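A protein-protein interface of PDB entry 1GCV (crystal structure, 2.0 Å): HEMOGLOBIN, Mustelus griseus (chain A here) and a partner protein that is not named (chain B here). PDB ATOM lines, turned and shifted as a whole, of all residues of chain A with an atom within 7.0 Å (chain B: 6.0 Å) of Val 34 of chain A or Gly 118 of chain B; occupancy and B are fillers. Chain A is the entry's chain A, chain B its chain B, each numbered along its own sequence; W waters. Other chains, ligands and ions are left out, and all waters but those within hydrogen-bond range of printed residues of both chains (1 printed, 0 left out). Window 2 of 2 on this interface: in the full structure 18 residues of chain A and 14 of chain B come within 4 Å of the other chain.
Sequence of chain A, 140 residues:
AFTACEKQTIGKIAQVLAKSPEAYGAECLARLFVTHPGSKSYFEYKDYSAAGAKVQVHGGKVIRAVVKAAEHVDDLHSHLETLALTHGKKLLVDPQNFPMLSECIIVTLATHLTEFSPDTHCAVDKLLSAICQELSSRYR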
ATOM      1  N   LEU A  29     -20.190  -1.820  17.355  1.00  0.00           N
ATOM      2  CA  LEU A  29     -21.007  -2.800  16.660  1.00  0.00           C
ATOM      3  C   LEU A  29     -20.363  -3.269  15.349  1.00  0.00           C
ATOM      4  O   LEU A  29     -20.462  -4.436  14.993  1.00  0.00           O
ATOM      5  CB  LEU A  29     -22.400  -2.217  16.398  1.00  0.00           C
ATOM      6  CG  LEU A  29     -23.238  -1.962  17.652  1.00  0.00           C
ATOM      7  CD1 LEU A  29     -24.466  -1.148  17.291  1.00  0.00           C
ATOM      8  CD2 LEU A  29     -23.637  -3.292  18.267  1.00  0.00           C
ATOM      9  N   ALA A  30     -19.699  -2.363  14.636  1.00  0.00           N
ATOM     10  CA  ALA A  30     -19.044  -2.716  13.374  1.00  0.00           C
ATOM     11  C   ALA A  30     -17.913  -3.718  13.595  1.00  0.00           C
ATOM     12  O   ALA A  30     -17.682  -4.598  12.766  1.00  0.00           O
ATOM     13  CB  ALA A  30     -18.501  -1.455  12.680  1.00  0.00           C
ATOM     14  N   ARG A  31     -17.198  -3.577  14.707  1.00  0.00           N
ATOM     15  CA  ARG A  31     -16.114  -4.497  15.009  1.00  0.00           C
ATOM     16  C   ARG A  31     -16.712  -5.855  15.327  1.00  0.00           C
ATOM     17  O   ARG A  31     -16.175  -6.887  14.924  1.00  0.00           O
ATOM     18  CB  ARG A  31     -15.301  -3.989  16.197  1.00  0.00           C
ATOM     19  CG  ARG A  31     -14.658  -2.658  15.929  1.00  0.00           C
ATOM     20  CD  ARG A  31     -13.557  -2.341  16.906  1.00  0.00           C
ATOM     21  NE  ARG A  31     -13.018  -1.019  16.612  1.00  0.00           N
ATOM     22  CZ  ARG A  31     -11.991  -0.802  15.804  1.00  0.00           C
ATOM     23  NH1 ARG A  31     -11.386  -1.823  15.211  1.00  0.00           N
ATOM     24  NH2 ARG A  31     -11.592   0.437  15.562  1.00  0.00           N
ATOM     25  N   LEU A  32     -17.831  -5.849  16.047  1.00  0.00           N
ATOM     26  CA  LEU A  32     -18.507  -7.088  16.419  1.00  0.00           C
ATOM     27  C   LEU A  32     -19.018  -7.807  15.178  1.00  0.00           C
ATOM     28  O   LEU A  32     -18.878  -9.022  15.053  1.00  0.00           O
ATOM     29  CB  LEU A  32     -19.682  -6.798  17.362  1.00  0.00           C
ATOM     30  CG  LEU A  32     -20.586  -7.980  17.742  1.00  0.00           C
ATOM     31  CD1 LEU A  32     -19.870  -8.884  18.721  1.00  0.00           C
ATOM     32  CD2 LEU A  32     -21.885  -7.462  18.348  1.00  0.00           C
ATOM     33  N   PHE A  33     -19.605  -7.052  14.258  1.00  0.00           N
ATOM     34  CA  PHE A  33     -20.141  -7.640  13.041  1.00  0.00           C
ATOM     35  C   PHE A  33     -19.032  -8.197  12.152  1.00  0.00           C
ATOM     36  O   PHE A  33     -19.257  -9.132  11.391  1.00  0.00           O
ATOM     37  CB  PHE A  33     -20.974  -6.609  12.270  1.00  0.00           C
ATOM     38  CG  PHE A  33     -22.229  -6.168  12.991  1.00  0.00           C
ATOM     39  CD1 PHE A  33     -22.949  -7.055  13.784  1.00  0.00           C
ATOM     40  CD2 PHE A  33     -22.686  -4.858  12.879  1.00  0.00           C
ATOM     41  CE1 PHE A  33     -24.111  -6.639  14.457  1.00  0.00           C
ATOM     42  CE2 PHE A  33     -23.839  -4.435  13.543  1.00  0.00           C
ATOM     43  CZ  PHE A  33     -24.551  -5.330  14.336  1.00  0.00           C
ATOM     44  N   VAL A  34     -17.832  -7.634  12.246  1.00  0.00           N
ATOM     45  CA  VAL A  34     -16.722  -8.117  11.429  1.00  0.00           C
ATOM     46  C   VAL A  34     -16.082  -9.345  12.063  1.00  0.00           C
ATOM     47  O   VAL A  34     -15.788 -10.327  11.379  1.00  0.00           O
ATOM     48  CB  VAL A  34     -15.626  -7.031  11.243  1.00  0.00           C
ATOM     49  CG1 VAL A  34     -14.304  -7.679  10.849  1.00  0.00           C
ATOM     50  CG2 VAL A  34     -16.049  -6.037  10.171  1.00  0.00           C
ATOM     51  N   THR A  35     -15.876  -9.291  13.373  1.00  0.00           N
ATOM     52  CA  THR A  35     -15.244 -10.394  14.084  1.00  0.00           C
ATOM     53  C   THR A  35     -16.161 -11.562  14.468  1.00  0.00           C
ATOM     54  O   THR A  35     -15.704 -12.698  14.591  1.00  0.00           O
ATOM     55  CB  THR A  35     -14.508  -9.873  15.341  1.00  0.00           C
ATOM     56  OG1 THR A  35     -15.437  -9.241  16.231  1.00  0.00           O
ATOM     57  CG2 THR A  35     -13.453  -8.862  14.931  1.00  0.00           C
ATOM     58  N   HIS A  36     -17.448 -11.284  14.659  1.00  0.00           N
ATOM     59  CA  HIS A  36     -18.420 -12.326  15.012  1.00  0.00           C
ATOM     60  C   HIS A  36     -19.657 -12.114  14.153  1.00  0.00           C
ATOM     61  O   HIS A  36     -20.686 -11.626  14.626  1.00  0.00           O
ATOM     62  CB  HIS A  36     -18.796 -12.238  16.494  1.00  0.00           C
ATOM     63  CG  HIS A  36     -17.660 -12.533  17.420  1.00  0.00           C
ATOM     64  ND1 HIS A  36     -16.960 -11.543  18.078  1.00  0.00           N
ATOM     65  CD2 HIS A  36     -17.096 -13.705  17.793  1.00  0.00           C
ATOM     66  CE1 HIS A  36     -16.013 -12.093  18.816  1.00  0.00           C
ATOM     67  NE2 HIS A  36     -16.074 -13.404  18.662  1.00  0.00           N
ATOM     68  N   PRO A  37     -19.570 -12.499  12.871  1.00  0.00           N
ATOM     69  CA  PRO A  37     -20.648 -12.367  11.882  1.00  0.00           C
ATOM     70  C   PRO A  37     -21.996 -12.933  12.323  1.00  0.00           C
ATOM     71  O   PRO A  37     -23.044 -12.424  11.934  1.00  0.00           O
ATOM     72  CB  PRO A  37     -20.099 -13.085  10.649  1.00  0.00           C
ATOM     73  CG  PRO A  37     -18.620 -13.095  10.833  1.00  0.00           C
ATOM     74  CD  PRO A  37     -18.375 -13.150  12.306  1.00  0.00           C
ATOM     75  N   SER A  39     -23.473 -12.566  14.904  1.00  0.00           N
ATOM     76  CA  SER A  39     -24.234 -11.571  15.640  1.00  0.00           C
ATOM     77  C   SER A  39     -25.063 -10.673  14.723  1.00  0.00           C
ATOM     78  O   SER A  39     -25.936  -9.946  15.189  1.00  0.00           O
ATOM     79  CB  SER A  39     -23.300 -10.728  16.521  1.00  0.00           C
ATOM     80  OG  SER A  39     -22.424  -9.937  15.737  1.00  0.00           O
ATOM     81  N   LYS A  40     -24.801 -10.725  13.419  1.00  0.00           N
ATOM     82  CA  LYS A  40     -25.560  -9.914  12.476  1.00  0.00           C
ATOM     83  C   LYS A  40     -26.966 -10.477  12.370  1.00  0.00           C
ATOM     84  O   LYS A  40     -27.888  -9.806  11.922  1.00  0.00           O
ATOM     85  CB  LYS A  40     -24.916  -9.945  11.092  1.00  0.00           C
ATOM     86  CG  LYS A  40     -23.506  -9.406  11.045  1.00  0.00           C
ATOM     87  CD  LYS A  40     -23.240  -8.691   9.736  1.00  0.00           C
ATOM     88  CE  LYS A  40     -22.413  -9.540   8.786  1.00  0.00           C
ATOM     89  NZ  LYS A  40     -22.428  -8.975   7.407  1.00  0.00           N
ATOM     90  N   TYR A  48     -23.719  -2.784   7.558  1.00  0.00           N
ATOM     91  CA  TYR A  48     -23.248  -3.225   8.865  1.00  0.00           C
ATOM     92  C   TYR A  48     -21.942  -2.538   9.232  1.00  0.00           C
ATOM     93  O   TYR A  48     -21.231  -2.978  10.134  1.00  0.00           O
ATOM     94  CB  TYR A  48     -23.056  -4.741   8.873  1.00  0.00           C
ATOM     95  CG  TYR A  48     -24.358  -5.505   8.840  1.00  0.00           C
ATOM     96  CD1 TYR A  48     -25.130  -5.653   9.991  1.00  0.00           C
ATOM     97  CD2 TYR A  48     -24.824  -6.071   7.652  1.00  0.00           C
ATOM     98  CE1 TYR A  48     -26.334  -6.345   9.966  1.00  0.00           C
ATOM     99  CE2 TYR A  48     -26.027  -6.764   7.614  1.00  0.00           C
ATOM    100  CZ  TYR A  48     -26.776  -6.898   8.773  1.00  0.00           C
ATOM    101  OH  TYR A  48     -27.963  -7.588   8.736  1.00  0.00           O
ATOM    102  N   CYS A 104     -15.201  -5.760  21.943  1.00  0.00           N
ATOM    103  CA  CYS A 104     -15.166  -4.782  20.857  1.00  0.00           C
ATOM    104  C   CYS A 104     -15.250  -3.354  21.384  1.00  0.00           C
ATOM    105  O   CYS A 104     -14.744  -2.427  20.753  1.00  0.00           O
ATOM    106  CB  CYS A 104     -16.294  -5.051  19.868  1.00  0.00           C
ATOM    107  SG  CYS A 104     -15.975  -6.506  18.872  1.00  0.00           S
ATOM    108  N   THR B 113      -8.947  -0.159  11.764  1.00  0.00           N
ATOM    109  CA  THR B 113     -10.355  -0.270  11.408  1.00  0.00           C
ATOM    110  C   THR B 113     -10.940  -1.651  11.681  1.00  0.00           C
ATOM    111  O   THR B 113     -10.201  -2.619  11.865  1.00  0.00           O
ATOM    112  CB  THR B 113     -10.551   0.039   9.913  1.00  0.00           C
ATOM    113  OG1 THR B 113      -9.951  -1.001   9.124  1.00  0.00           O
ATOM    114  CG2 THR B 113      -9.905   1.365   9.560  1.00  0.00           C
ATOM    115  N   PRO B 114     -12.282  -1.748  11.751  1.00  0.00           N
ATOM    116  CA  PRO B 114     -12.940  -3.036  11.996  1.00  0.00           C
ATOM    117  C   PRO B 114     -12.448  -4.101  11.014  1.00  0.00           C
ATOM    118  O   PRO B 114     -12.281  -5.266  11.377  1.00  0.00           O
ATOM    119  CB  PRO B 114     -14.427  -2.719  11.816  1.00  0.00           C
ATOM    120  CG  PRO B 114     -14.532  -1.280  12.203  1.00  0.00           C
ATOM    121  CD  PRO B 114     -13.257  -0.645  11.680  1.00  0.00           C
ATOM    122  N   HIS B 115     -12.208  -3.687   9.771  1.00  0.00           N
ATOM    123  CA  HIS B 115     -11.722  -4.596   8.739  1.00  0.00           C
ATOM    124  C   HIS B 115     -10.306  -5.077   9.072  1.00  0.00           C
ATOM    125  O   HIS B 115     -10.012  -6.274   8.979  1.00  0.00           O
ATOM    126  CB  HIS B 115     -11.732  -3.908   7.369  1.00  0.00           C
ATOM    127  CG  HIS B 115     -11.169  -4.753   6.270  1.00  0.00           C
ATOM    128  ND1 HIS B 115      -9.955  -4.487   5.674  1.00  0.00           N
ATOM    129  CD2 HIS B 115     -11.634  -5.885   5.690  1.00  0.00           C
ATOM    130  CE1 HIS B 115      -9.695  -5.420   4.776  1.00  0.00           C
ATOM    131  NE2 HIS B 115     -10.698  -6.280   4.766  1.00  0.00           N
ATOM    132  N   ILE B 116      -9.436  -4.148   9.460  1.00  0.00           N
ATOM    133  CA  ILE B 116      -8.065  -4.500   9.825  1.00  0.00           C
ATOM    134  C   ILE B 116      -8.062  -5.401  11.069  1.00  0.00           C
ATOM    135  O   ILE B 116      -7.277  -6.347  11.151  1.00  0.00           O
ATOM    136  CB  ILE B 116      -7.212  -3.245  10.108  1.00  0.00           C
ATOM    137  CG1 ILE B 116      -7.100  -2.391   8.844  1.00  0.00           C
ATOM    138  CG2 ILE B 116      -5.826  -3.657  10.576  1.00  0.00           C
ATOM    139  CD1 ILE B 116      -6.420  -3.095   7.686  1.00  0.00           C
ATOM    140  N   GLN B 117      -8.935  -5.104  12.035  1.00  0.00           N
ATOM    141  CA  GLN B 117      -9.028  -5.914  13.250  1.00  0.00           C
ATOM    142  C   GLN B 117      -9.438  -7.327  12.855  1.00  0.00           C
ATOM    143  O   GLN B 117      -8.954  -8.304  13.426  1.00  0.00           O
ATOM    144  CB  GLN B 117     -10.064  -5.342  14.224  1.00  0.00           C
ATOM    145  CG  GLN B 117     -10.362  -6.272  15.411  1.00  0.00           C
ATOM    146  CD  GLN B 117     -11.406  -5.726  16.375  1.00  0.00           C
ATOM    147  OE1 GLN B 117     -11.957  -4.647  16.172  1.00  0.00           O
ATOM    148  NE2 GLN B 117     -11.680  -6.480  17.436  1.00  0.00           N
ATOM    149  N   GLY B 118     -10.338  -7.423  11.878  1.00  0.00           N
ATOM    150  CA  GLY B 118     -10.793  -8.717  11.400  1.00  0.00           C
ATOM    151  C   GLY B 118      -9.660  -9.573  10.852  1.00  0.00           C
ATOM    152  O   GLY B 118      -9.657 -10.784  11.040  1.00  0.00           O
ATOM    153  N   ILE B 119      -8.694  -8.949  10.176  1.00  0.00           N
ATOM    154  CA  ILE B 119      -7.563  -9.679   9.617  1.00  0.00           C
ATOM    155  C   ILE B 119      -6.682 -10.246  10.736  1.00  0.00           C
ATOM    156  O   ILE B 119      -6.254 -11.397  10.682  1.00  0.00           O
ATOM    157  CB  ILE B 119      -6.707  -8.766   8.711  1.00  0.00           C
ATOM    158  CG1 ILE B 119      -7.538  -8.298   7.514  1.00  0.00           C
ATOM    159  CG2 ILE B 119      -5.467  -9.514   8.228  1.00  0.00           C
ATOM    160  CD1 ILE B 119      -6.846  -7.257   6.653  1.00  0.00           C
ATOM    161  N   TRP B 120      -6.419  -9.428  11.748  1.00  0.00           N
ATOM    162  CA  TRP B 120      -5.604  -9.846  12.880  1.00  0.00           C
ATOM    163  C   TRP B 120      -6.312 -10.901  13.720  1.00  0.00           C
ATOM    164  O   TRP B 120      -5.691 -11.840  14.210  1.00  0.00           O
ATOM    165  CB  TRP B 120      -5.262  -8.631  13.731  1.00  0.00           C
ATOM    166  CG  TRP B 120      -4.192  -7.838  13.091  1.00  0.00           C
ATOM    167  CD1 TRP B 120      -4.340  -6.714  12.326  1.00  0.00           C
ATOM    168  CD2 TRP B 120      -2.798  -8.145  13.091  1.00  0.00           C
ATOM    169  NE1 TRP B 120      -3.120  -6.306  11.846  1.00  0.00           N
ATOM    170  CE2 TRP B 120      -2.155  -7.167  12.301  1.00  0.00           C
ATOM    171  CE3 TRP B 120      -2.026  -9.156  13.680  1.00  0.00           C
ATOM    172  CZ2 TRP B 120      -0.773  -7.168  12.087  1.00  0.00           C
ATOM    173  CZ3 TRP B 120      -0.653  -9.158  13.467  1.00  0.00           C
ATOM    174  CH2 TRP B 120      -0.042  -8.168  12.676  1.00  0.00           C
ATOM    175  N   ASP B 121      -7.617 -10.741  13.883  1.00  0.00           N
ATOM    176  CA  ASP B 121      -8.409 -11.699  14.646  1.00  0.00           C
ATOM    177  C   ASP B 121      -8.284 -13.054  13.963  1.00  0.00           C
ATOM    178  O   ASP B 121      -8.099 -14.083  14.609  1.00  0.00           O
ATOM    179  CB  ASP B 121      -9.875 -11.260  14.658  1.00  0.00           C
ATOM    180  CG  ASP B 121     -10.746 -12.155  15.511  1.00  0.00           C
ATOM    181  OD1 ASP B 121     -11.452 -13.010  14.948  1.00  0.00           O
ATOM    182  OD2 ASP B 121     -10.728 -12.001  16.747  1.00  0.00           O
ATOM    183  N   LYS B 122      -8.385 -13.032  12.640  1.00  0.00           N
ATOM    184  CA  LYS B 122      -8.291 -14.233  11.826  1.00  0.00           C
ATOM    185  C   LYS B 122      -6.916 -14.854  11.969  1.00  0.00           C
ATOM    186  O   LYS B 122      -6.784 -16.064  12.134  1.00  0.00           O
ATOM    187  CB  LYS B 122      -8.550 -13.882  10.364  1.00  0.00           C
ATOM    188  CG  LYS B 122      -8.549 -15.069   9.437  1.00  0.00           C
ATOM    189  CD  LYS B 122      -8.591 -14.609   7.993  1.00  0.00           C
ATOM    190  CE  LYS B 122      -9.221 -15.660   7.105  1.00  0.00           C
ATOM    191  NZ  LYS B 122      -8.656 -15.616   5.733  1.00  0.00           N
ATOM    192  N   PHE B 123      -5.885 -14.019  11.911  1.00  0.00           N
ATOM    193  CA  PHE B 123      -4.526 -14.512  12.043  1.00  0.00           C
ATOM    194  C   PHE B 123      -4.285 -15.148  13.407  1.00  0.00           C
ATOM    195  O   PHE B 123      -3.707 -16.230  13.489  1.00  0.00           O
ATOM    196  CB  PHE B 123      -3.515 -13.387  11.825  1.00  0.00           C
ATOM    197  CG  PHE B 123      -2.081 -13.839  11.907  1.00  0.00           C
ATOM    198  CD1 PHE B 123      -1.576 -14.762  10.993  1.00  0.00           C
ATOM    199  CD2 PHE B 123      -1.241 -13.357  12.907  1.00  0.00           C
ATOM    200  CE1 PHE B 123      -0.255 -15.199  11.074  1.00  0.00           C
ATOM    201  CE2 PHE B 123       0.084 -13.789  12.993  1.00  0.00           C
ATOM    202  CZ  PHE B 123       0.576 -14.712  12.074  1.00  0.00           C
HETATM  203  O   HOH W   1     -12.851 -12.223  19.279  1.00  0.00           O
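Printed residues of chain B that touch a printed residue of chain A: Thr 113, Pro 114, Gln 117 and Gly 118.
Hydrophobic or aromatic side chains of chain A that line the printed part of chain B: Val 34.
Among the printed residues, 7 pairs touch across the chains.
The guanidinium group of Arg 31 of chain A sits close to the side-chain amide oxygen of Gln 117 of chain B (3.0 Å).
Water W1 lies within hydrogen-bond range of the side-chain carboxylate (OD2) of Asp 121 of chain B and a ring nitrogen (NE2) of His 36 of chain A.
The side-chain hydroxyl (OG1) of Thr 35 of chain A lies within hydrogen-bond range of a ring nitrogen (ND1) of His 36 of chain A.
OG1 of Thr 113 of chain B sits close to N of Ile 116 of chain B (3.2 Å).
The backbone carbonyl oxygen of Arg 31 of chain A is in hydrogen-bond range of the side-chain hydroxyl of Thr 35 of chain A (2.8 Å).
Of the printed residues of chain B, Val 34 of chain A touches Pro 114 and Gly 118.
Of chain A, only Val 34 (3.7 Å) comes within 4 Å of Gly 118 of chain B.
Of the printed residues of chain B, Ala 30 of chain A touches Pro 114.
Of the printed residues of chain B, Thr 35 of chain A touches Gln 117.
Printed residues of chain A within 4 Å of Thr 113 of chain B: Arg 31 (3.6 Å).
Of the printed residues of chain B, Arg 31 of chain A touches Thr 113, Pro 114 and Gln 117.
Of the printed residues of chain A, Pro 114 of chain B touches Ala 30 (3.9 Å), Arg 31 (3.6 Å) and Val 34 (3.2 Å).
Phe 33 of chain A touches none of the printed residues of chain B.
Phe 123 of chain B touches none of the printed residues of chain A.
The nearest residue of chain B that does not touch Val 34 of chain A is His 115 of chain B (4.5 Å).
The nearest printed residue of chain B that does not touch Arg 31 of chain A is His 115 of chain B (5.8 Å).
Ala 30 of chain A touches Pro 114 of chain B.
NH1 of Arg 31 of chain A touches C of Thr 113 of chain B, 3.6 Å away.
Pro 114 of chain B touches Arg 31 of chain A.
CG1 of Val 34 of chain A touches O of Pro 114 of chain B, 3.2 Å away.
Gly 118 of chain B touches Val 34 of chain A (CA to CG1, 3.7 Å).
Thr 35 of chain A touches Gln 117 of chain B (CG2 to NE2, 3.9 Å).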
